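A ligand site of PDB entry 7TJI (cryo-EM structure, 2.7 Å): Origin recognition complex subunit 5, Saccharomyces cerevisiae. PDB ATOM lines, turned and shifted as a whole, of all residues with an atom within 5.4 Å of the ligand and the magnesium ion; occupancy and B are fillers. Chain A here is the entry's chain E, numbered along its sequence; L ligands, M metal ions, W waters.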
ATOM      1  N   VAL A   8       4.763  28.402 -36.474  1.00  0.00           N
ATOM      2  CA  VAL A   8       4.285  28.499 -35.106  1.00  0.00           C
ATOM      3  C   VAL A   8       4.093  29.972 -34.791  1.00  0.00           C
ATOM      4  O   VAL A   8       4.957  30.798 -35.117  1.00  0.00           O
ATOM      5  CB  VAL A   8       5.253  27.824 -34.121  1.00  0.00           C
ATOM      6  CG1 VAL A   8       4.632  27.707 -32.737  1.00  0.00           C
ATOM      7  CG2 VAL A   8       5.637  26.457 -34.628  1.00  0.00           C
ATOM      8  N   ALA A   9       2.971  30.300 -34.134  1.00  0.00           N
ATOM      9  CA  ALA A   9       2.375  31.629 -34.187  1.00  0.00           C
ATOM     10  C   ALA A   9       3.270  32.708 -33.580  1.00  0.00           C
ATOM     11  O   ALA A   9       3.384  33.813 -34.140  1.00  0.00           O
ATOM     12  CB  ALA A   9       1.015  31.629 -33.486  1.00  0.00           C
ATOM     13  N   PHE A  10       3.917  32.413 -32.463  1.00  0.00           N
ATOM     14  CA  PHE A  10       4.808  33.394 -31.831  1.00  0.00           C
ATOM     15  C   PHE A  10       6.169  32.791 -31.526  1.00  0.00           C
ATOM     16  O   PHE A  10       6.870  33.285 -30.639  1.00  0.00           O
ATOM     17  CB  PHE A  10       4.159  33.968 -30.570  1.00  0.00           C
ATOM     18  CG  PHE A  10       2.755  34.465 -30.771  1.00  0.00           C
ATOM     19  CD1 PHE A  10       2.523  35.729 -31.291  1.00  0.00           C
ATOM     20  CD2 PHE A  10       1.665  33.658 -30.448  1.00  0.00           C
ATOM     21  CE1 PHE A  10       1.235  36.185 -31.478  1.00  0.00           C
ATOM     22  CE2 PHE A  10       0.377  34.114 -30.636  1.00  0.00           C
ATOM     23  CZ  PHE A  10       0.162  35.377 -31.151  1.00  0.00           C
ATOM     24  N   ARG A  11       6.555  31.747 -32.247  1.00  0.00           N
ATOM     25  CA  ARG A  11       7.839  31.071 -32.079  1.00  0.00           C
ATOM     26  C   ARG A  11       8.553  30.970 -33.416  1.00  0.00           C
ATOM     27  O   ARG A  11       9.175  29.940 -33.735  1.00  0.00           O
ATOM     28  CB  ARG A  11       7.655  29.691 -31.463  1.00  0.00           C
ATOM     29  CG  ARG A  11       6.883  29.664 -30.148  1.00  0.00           C
ATOM     30  CD  ARG A  11       7.778  29.882 -28.955  1.00  0.00           C
ATOM     31  NE  ARG A  11       7.979  31.288 -28.640  1.00  0.00           N
ATOM     32  CZ  ARG A  11       8.156  31.773 -27.428  1.00  0.00           C
ATOM     33  NH1 ARG A  11       8.164  30.989 -26.368  1.00  0.00           N
ATOM     34  NH2 ARG A  11       8.345  33.079 -27.266  1.00  0.00           N
ATOM     35  N   GLY A  37      13.739  27.206 -21.708  1.00  0.00           N
ATOM     36  CA  GLY A  37      12.617  28.080 -21.453  1.00  0.00           C
ATOM     37  C   GLY A  37      11.852  27.592 -20.253  1.00  0.00           C
ATOM     38  O   GLY A  37      11.992  26.425 -19.843  1.00  0.00           O
ATOM     39  N   TYR A  38      11.023  28.466 -19.699  1.00  0.00           N
ATOM     40  CA  TYR A  38      10.246  28.105 -18.529  1.00  0.00           C
ATOM     41  C   TYR A  38       8.966  27.398 -18.956  1.00  0.00           C
ATOM     42  O   TYR A  38       8.753  27.104 -20.133  1.00  0.00           O
ATOM     43  CB  TYR A  38       9.999  29.344 -17.661  1.00  0.00           C
ATOM     44  CG  TYR A  38      11.261  29.765 -16.962  1.00  0.00           C
ATOM     45  CD1 TYR A  38      11.626  29.198 -15.746  1.00  0.00           C
ATOM     46  CD2 TYR A  38      12.135  30.687 -17.540  1.00  0.00           C
ATOM     47  CE1 TYR A  38      12.793  29.560 -15.113  1.00  0.00           C
ATOM     48  CE2 TYR A  38      13.310  31.048 -16.914  1.00  0.00           C
ATOM     49  CZ  TYR A  38      13.628  30.488 -15.705  1.00  0.00           C
ATOM     50  OH  TYR A  38      14.788  30.850 -15.065  1.00  0.00           O
ATOM     51  N   SER A  39       8.105  27.104 -17.977  1.00  0.00           N
ATOM     52  CA  SER A  39       6.919  26.294 -18.230  1.00  0.00           C
ATOM     53  C   SER A  39       5.916  27.049 -19.085  1.00  0.00           C
ATOM     54  O   SER A  39       5.675  28.237 -18.890  1.00  0.00           O
ATOM     55  CB  SER A  39       6.274  25.859 -16.920  1.00  0.00           C
ATOM     56  OG  SER A  39       6.937  24.735 -16.372  1.00  0.00           O
ATOM     57  N   GLY A  40       5.319  26.329 -20.036  1.00  0.00           N
ATOM     58  CA  GLY A  40       4.358  26.907 -20.951  1.00  0.00           C
ATOM     59  C   GLY A  40       4.928  27.948 -21.886  1.00  0.00           C
ATOM     60  O   GLY A  40       4.260  28.940 -22.177  1.00  0.00           O
ATOM     61  N   THR A  41       6.154  27.751 -22.357  1.00  0.00           N
ATOM     62  CA  THR A  41       6.758  28.629 -23.345  1.00  0.00           C
ATOM     63  C   THR A  41       6.772  28.016 -24.735  1.00  0.00           C
ATOM     64  O   THR A  41       7.373  28.577 -25.648  1.00  0.00           O
ATOM     65  CB  THR A  41       8.176  29.019 -22.926  1.00  0.00           C
ATOM     66  OG1 THR A  41       8.894  27.852 -22.515  1.00  0.00           O
ATOM     67  CG2 THR A  41       8.124  30.003 -21.782  1.00  0.00           C
ATOM     68  N   GLY A  42       6.125  26.868 -24.910  1.00  0.00           N
ATOM     69  CA  GLY A  42       5.994  26.276 -26.223  1.00  0.00           C
ATOM     70  C   GLY A  42       7.171  25.491 -26.722  1.00  0.00           C
ATOM     71  O   GLY A  42       7.311  25.321 -27.932  1.00  0.00           O
ATOM     72  N   LYS A  43       8.042  25.004 -25.836  1.00  0.00           N
ATOM     73  CA  LYS A  43       9.196  24.227 -26.270  1.00  0.00           C
ATOM     74  C   LYS A  43       8.785  22.892 -26.863  1.00  0.00           C
ATOM     75  O   LYS A  43       9.202  22.535 -27.979  1.00  0.00           O
ATOM     76  CB  LYS A  43      10.148  24.014 -25.087  1.00  0.00           C
ATOM     77  CG  LYS A  43      10.590  25.287 -24.397  1.00  0.00           C
ATOM     78  CD  LYS A  43      11.517  24.988 -23.229  1.00  0.00           C
ATOM     79  CE  LYS A  43      10.788  24.245 -22.110  1.00  0.00           C
ATOM     80  NZ  LYS A  43       9.716  25.019 -21.440  1.00  0.00           N
ATOM     81  N   THR A  44       7.946  22.142 -26.152  1.00  0.00           N
ATOM     82  CA  THR A  44       7.458  20.856 -26.635  1.00  0.00           C
ATOM     83  C   THR A  44       6.592  21.028 -27.870  1.00  0.00           C
ATOM     84  O   THR A  44       6.700  20.245 -28.825  1.00  0.00           O
ATOM     85  CB  THR A  44       6.662  20.140 -25.533  1.00  0.00           C
ATOM     86  OG1 THR A  44       7.430  20.144 -24.320  1.00  0.00           O
ATOM     87  CG2 THR A  44       6.365  18.703 -25.915  1.00  0.00           C
ATOM     88  N   TYR A  45       5.744  22.064 -27.879  1.00  0.00           N
ATOM     89  CA  TYR A  45       4.861  22.336 -29.010  1.00  0.00           C
ATOM     90  C   TYR A  45       5.647  22.653 -30.279  1.00  0.00           C
ATOM     91  O   TYR A  45       5.369  22.098 -31.348  1.00  0.00           O
ATOM     92  CB  TYR A  45       3.907  23.475 -28.635  1.00  0.00           C
ATOM     93  CG  TYR A  45       2.867  23.830 -29.689  1.00  0.00           C
ATOM     94  CD1 TYR A  45       1.665  23.143 -29.775  1.00  0.00           C
ATOM     95  CD2 TYR A  45       3.084  24.875 -30.576  1.00  0.00           C
ATOM     96  CE1 TYR A  45       0.729  23.466 -30.723  1.00  0.00           C
ATOM     97  CE2 TYR A  45       2.155  25.212 -31.530  1.00  0.00           C
ATOM     98  CZ  TYR A  45       0.980  24.511 -31.601  1.00  0.00           C
ATOM     99  OH  TYR A  45       0.051  24.848 -32.555  1.00  0.00           O
ATOM    100  N   THR A  46       6.660  23.508 -30.167  1.00  0.00           N
ATOM    101  CA  THR A  46       7.471  23.884 -31.328  1.00  0.00           C
ATOM    102  C   THR A  46       8.329  22.721 -31.817  1.00  0.00           C
ATOM    103  O   THR A  46       8.448  22.515 -33.036  1.00  0.00           O
ATOM    104  CB  THR A  46       8.356  25.087 -30.995  1.00  0.00           C
ATOM    105  OG1 THR A  46       7.639  25.988 -30.156  1.00  0.00           O
ATOM    106  CG2 THR A  46       8.794  25.797 -32.256  1.00  0.00           C
ATOM    107  N   ASP A 133      13.407  15.676 -23.188  1.00  0.00           N
ATOM    108  CA  ASP A 133      12.505  16.793 -22.921  1.00  0.00           C
ATOM    109  C   ASP A 133      12.342  16.953 -21.413  1.00  0.00           C
ATOM    110  O   ASP A 133      11.503  16.300 -20.795  1.00  0.00           O
ATOM    111  CB  ASP A 133      11.156  16.563 -23.597  1.00  0.00           C
ATOM    112  CG  ASP A 133      10.419  17.852 -23.892  1.00  0.00           C
ATOM    113  OD1 ASP A 133      10.420  18.754 -23.042  1.00  0.00           O
ATOM    114  OD2 ASP A 133       9.825  17.964 -24.977  1.00  0.00           O
ATOM    115  N   LEU A 171      14.623  23.926 -18.168  1.00  0.00           N
ATOM    116  CA  LEU A 171      13.754  24.907 -17.537  1.00  0.00           C
ATOM    117  C   LEU A 171      14.529  26.077 -16.933  1.00  0.00           C
ATOM    118  O   LEU A 171      14.177  27.229 -17.162  1.00  0.00           O
ATOM    119  CB  LEU A 171      12.908  24.232 -16.449  1.00  0.00           C
ATOM    120  CG  LEU A 171      11.678  23.448 -16.908  1.00  0.00           C
ATOM    121  CD1 LEU A 171      11.084  22.650 -15.754  1.00  0.00           C
ATOM    122  CD2 LEU A 171      10.642  24.354 -17.525  1.00  0.00           C
ATOM    123  N   TYR A 192       5.677  34.253 -22.745  1.00  0.00           N
ATOM    124  CA  TYR A 192       4.774  34.881 -23.699  1.00  0.00           C
ATOM    125  C   TYR A 192       4.242  36.211 -23.167  1.00  0.00           C
ATOM    126  O   TYR A 192       4.203  36.460 -21.961  1.00  0.00           O
ATOM    127  CB  TYR A 192       3.607  33.957 -24.023  1.00  0.00           C
ATOM    128  CG  TYR A 192       3.929  32.796 -24.927  1.00  0.00           C
ATOM    129  CD1 TYR A 192       4.398  33.004 -26.213  1.00  0.00           C
ATOM    130  CD2 TYR A 192       3.760  31.485 -24.494  1.00  0.00           C
ATOM    131  CE1 TYR A 192       4.688  31.950 -27.046  1.00  0.00           C
ATOM    132  CE2 TYR A 192       4.047  30.423 -25.315  1.00  0.00           C
ATOM    133  CZ  TYR A 192       4.513  30.652 -26.589  1.00  0.00           C
ATOM    134  OH  TYR A 192       4.795  29.598 -27.416  1.00  0.00           O
ATOM    135  N   ILE A 200      -3.162  32.395 -28.053  1.00  0.00           N
ATOM    136  CA  ILE A 200      -2.950  30.963 -27.912  1.00  0.00           C
ATOM    137  C   ILE A 200      -4.131  30.315 -27.218  1.00  0.00           C
ATOM    138  O   ILE A 200      -4.594  29.236 -27.625  1.00  0.00           O
ATOM    139  CB  ILE A 200      -1.615  30.699 -27.175  1.00  0.00           C
ATOM    140  CG1 ILE A 200      -0.431  30.912 -28.130  1.00  0.00           C
ATOM    141  CG2 ILE A 200      -1.546  29.308 -26.570  1.00  0.00           C
ATOM    142  CD1 ILE A 200       0.874  31.192 -27.427  1.00  0.00           C
ATOM    143  N   MET A 203      -7.078  30.204 -29.760  1.00  0.00           N
ATOM    144  CA  MET A 203      -6.826  29.245 -30.824  1.00  0.00           C
ATOM    145  C   MET A 203      -6.673  27.817 -30.336  1.00  0.00           C
ATOM    146  O   MET A 203      -6.709  26.894 -31.166  1.00  0.00           O
ATOM    147  CB  MET A 203      -5.586  29.666 -31.619  1.00  0.00           C
ATOM    148  CG  MET A 203      -4.269  29.123 -31.073  1.00  0.00           C
ATOM    149  SD  MET A 203      -2.944  29.208 -32.293  1.00  0.00           S
ATOM    150  CE  MET A 203      -2.683  30.978 -32.371  1.00  0.00           C
ATOM    151  N   SER A 204      -6.502  27.589 -29.038  1.00  0.00           N
ATOM    152  CA  SER A 204      -6.400  26.239 -28.517  1.00  0.00           C
ATOM    153  C   SER A 204      -7.573  25.813 -27.659  1.00  0.00           C
ATOM    154  O   SER A 204      -7.695  24.620 -27.370  1.00  0.00           O
ATOM    155  CB  SER A 204      -5.100  26.089 -27.698  1.00  0.00           C
ATOM    156  OG  SER A 204      -5.024  27.058 -26.681  1.00  0.00           O
ATOM    157  N   ILE A 255      -0.065  29.730 -19.050  1.00  0.00           N
ATOM    158  CA  ILE A 255      -1.110  29.168 -19.894  1.00  0.00           C
ATOM    159  C   ILE A 255      -1.903  28.115 -19.130  1.00  0.00           C
ATOM    160  O   ILE A 255      -3.135  28.043 -19.251  1.00  0.00           O
ATOM    161  CB  ILE A 255      -0.484  28.600 -21.182  1.00  0.00           C
ATOM    162  CG1 ILE A 255       0.168  29.714 -22.004  1.00  0.00           C
ATOM    163  CG2 ILE A 255      -1.504  27.869 -22.043  1.00  0.00           C
ATOM    164  CD1 ILE A 255       0.853  29.246 -23.252  1.00  0.00           C
ATOM    165  N   PHE A 256      -1.222  27.314 -18.298  1.00  0.00           N
ATOM    166  CA  PHE A 256      -1.876  26.191 -17.632  1.00  0.00           C
ATOM    167  C   PHE A 256      -2.847  26.653 -16.550  1.00  0.00           C
ATOM    168  O   PHE A 256      -3.928  26.070 -16.387  1.00  0.00           O
ATOM    169  CB  PHE A 256      -0.810  25.257 -17.041  1.00  0.00           C
ATOM    170  CG  PHE A 256       0.077  24.624 -18.068  1.00  0.00           C
ATOM    171  CD1 PHE A 256      -0.398  23.596 -18.874  1.00  0.00           C
ATOM    172  CD2 PHE A 256       1.395  25.034 -18.231  1.00  0.00           C
ATOM    173  CE1 PHE A 256       0.414  23.006 -19.819  1.00  0.00           C
ATOM    174  CE2 PHE A 256       2.211  24.451 -19.171  1.00  0.00           C
ATOM    175  CZ  PHE A 256       1.728  23.437 -19.971  1.00  0.00           C
HETATM  176  P1  LIG L   1       6.766  22.523 -19.849  1.00  0.00           P
HETATM  177  O1  LIG L   1       8.102  23.011 -19.419  1.00  0.00           O
HETATM  178  O2  LIG L   1       5.722  22.596 -18.761  1.00  0.00           O
HETATM  179  O3  LIG L   1       6.782  21.122 -20.434  1.00  0.00           O
HETATM  180  P2  LIG L   1       6.476  23.792 -22.537  1.00  0.00           P
HETATM  181  O4  LIG L   1       7.314  24.995 -22.693  1.00  0.00           O
HETATM  182  O5  LIG L   1       7.028  22.545 -23.200  1.00  0.00           O
HETATM  183  O6  LIG L   1       6.193  23.434 -21.017  1.00  0.00           O
HETATM  184  P3  LIG L   1       4.038  23.338 -24.140  1.00  0.00           P
HETATM  185  O7  LIG L   1       3.574  22.017 -23.668  1.00  0.00           O
HETATM  186  O8  LIG L   1       4.799  23.273 -25.453  1.00  0.00           O
HETATM  187  O9  LIG L   1       5.010  24.029 -23.089  1.00  0.00           O
HETATM  188  O10 LIG L   1       2.864  24.369 -24.317  1.00  0.00           O
HETATM  189  C1  LIG L   1       1.655  24.280 -23.548  1.00  0.00           C
HETATM  190  C2  LIG L   1       0.472  24.119 -24.460  1.00  0.00           C
HETATM  191  O11 LIG L   1       0.010  25.423 -24.896  1.00  0.00           O
HETATM  192  C3  LIG L   1       0.735  23.341 -25.742  1.00  0.00           C
HETATM  193  O12 LIG L   1       0.542  21.948 -25.554  1.00  0.00           O
HETATM  194  C4  LIG L   1      -0.296  23.932 -26.708  1.00  0.00           C
HETATM  195  O13 LIG L   1      -1.588  23.346 -26.515  1.00  0.00           O
HETATM  196  C5  LIG L   1      -0.322  25.394 -26.275  1.00  0.00           C
HETATM  197  N1  LIG L   1       0.630  26.244 -26.992  1.00  0.00           N
HETATM  198  C6  LIG L   1       1.858  26.668 -26.551  1.00  0.00           C
HETATM  199  N2  LIG L   1       2.491  27.435 -27.395  1.00  0.00           N
HETATM  200  C7  LIG L   1       1.620  27.531 -28.467  1.00  0.00           C
HETATM  201  C8  LIG L   1       1.707  28.208 -29.707  1.00  0.00           C
HETATM  202  N3  LIG L   1       2.757  28.951 -30.078  1.00  0.00           N
HETATM  203  N4  LIG L   1       0.662  28.093 -30.552  1.00  0.00           N
HETATM  204  C9  LIG L   1      -0.384  27.356 -30.193  1.00  0.00           C
HETATM  205  N5  LIG L   1      -0.571  26.676 -29.054  1.00  0.00           N
HETATM  206  C10 LIG L   1       0.464  26.806 -28.237  1.00  0.00           C
HETATM  207 MG    MG M   1       7.249  20.177 -22.247  1.00  0.00          MG
HETATM  208  O   HOH W   1       7.586  17.923 -21.358  1.00  0.00           O
HETATM  209  O   HOH W   2       7.334  21.764 -16.278  1.00  0.00           O
HETATM  210  O   HOH W   3       9.215  20.960 -22.033  1.00  0.00           O
HETATM  211  O   HOH W   4       5.170  20.304 -22.562  1.00  0.00           O
HETATM  212  O   HOH W   5       5.904  18.854 -18.966  1.00  0.00           O
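N of Thr 44 is in hydrogen-bond range of O8 of the ligand (3.4 Å). An oxygen (O4) of the ligand is in hydrogen-bond range of the backbone NH of Lys 43. An oxygen (O4) of the ligand is in salt-bridge range of the side-chain amino group (NZ) of Lys 43. O8 of the ligand is in hydrogen-bond range of N of Tyr 45 (2.9 Å). N of Thr 41 lies within hydrogen-bond range of O4 of the ligand (3.0 Å). The side-chain hydroxyl of Thr 41 is in hydrogen-bond range of an oxygen (O4) of the ligand, at 3.3 Å. O4 of the ligand is in hydrogen-bond range of N of Gly 42, at 3.1 Å. A nitrogen (N2) of the ligand lies within hydrogen-bond range of the side-chain hydroxyl (OH) of Tyr 192 (3.2 Å). The backbone NH of Gly 40 sits at hydrogen-bond distance from an oxygen (O6) of the ligand, 3.2 Å away. The side-chain hydroxyl (OG) of Ser 39 sits at hydrogen-bond distance from an oxygen (O2) of the ligand (3.4 Å).
Merely in contact with the magnesium ion: Asp 133. Of the 22 residues printed, 2 come within 4 Å of the magnesium ion.
Merely in contact with the ligand: Leu 171 (3.4 Å), Val 8 (3.5 Å), Tyr 38 (3.6 Å), Ile 200 (3.6 Å), Phe 256 (3.7 Å) and Met 203 (3.8 Å). Hydrophobic or aromatic side chains that line the ligand: Val 8, Tyr 45, Leu 171, Tyr 192, Ile 200, Met 203 and Phe 256.
The side-chain hydroxyl (OG1) of Thr 44 sits close to the side-chain carboxylate (OD2) of Asp 133 (3.3 Å). OG1 of Thr 41 lies within hydrogen-bond range of NZ of Lys 43, at 3.1 Å. NZ of Lys 43 is in hydrogen-bond range of O of Tyr 38, at 2.6 Å. The side-chain amino group (NZ) of Lys 43 sits at hydrogen-bond distance from the backbone carbonyl oxygen (O) of Gly 37 (3.1 Å). O of Thr 41 lies within hydrogen-bond range of OH of Tyr 192. The backbone carbonyl oxygen of Tyr 38 lies within hydrogen-bond range of the side-chain hydroxyl of Thr 41. The guanidinium group of Arg 11 sits at hydrogen-bond distance from the backbone carbonyl oxygen of Thr 41, at 2.6 Å. The backbone carbonyl oxygen (O) of Ile 200 is in hydrogen-bond range of the side-chain hydroxyl (OG) of Ser 204 (2.4 Å).
Water W2 lies within hydrogen-bond range of the side-chain hydroxyl (OG) of Ser 39 (3.0 Å) and an oxygen (O2) of the ligand (3.1 Å).
The magnesium ion is bound by OG1 of Thr 44 (2.1 Å). O3 of the ligand is bound to the magnesium ion. Water W4 is bound to the magnesium ion, at 2.1 Å. Water W3 is bound to the magnesium ion. Water W1 is bound to the magnesium ion. O5 of the ligand binds the magnesium ion.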
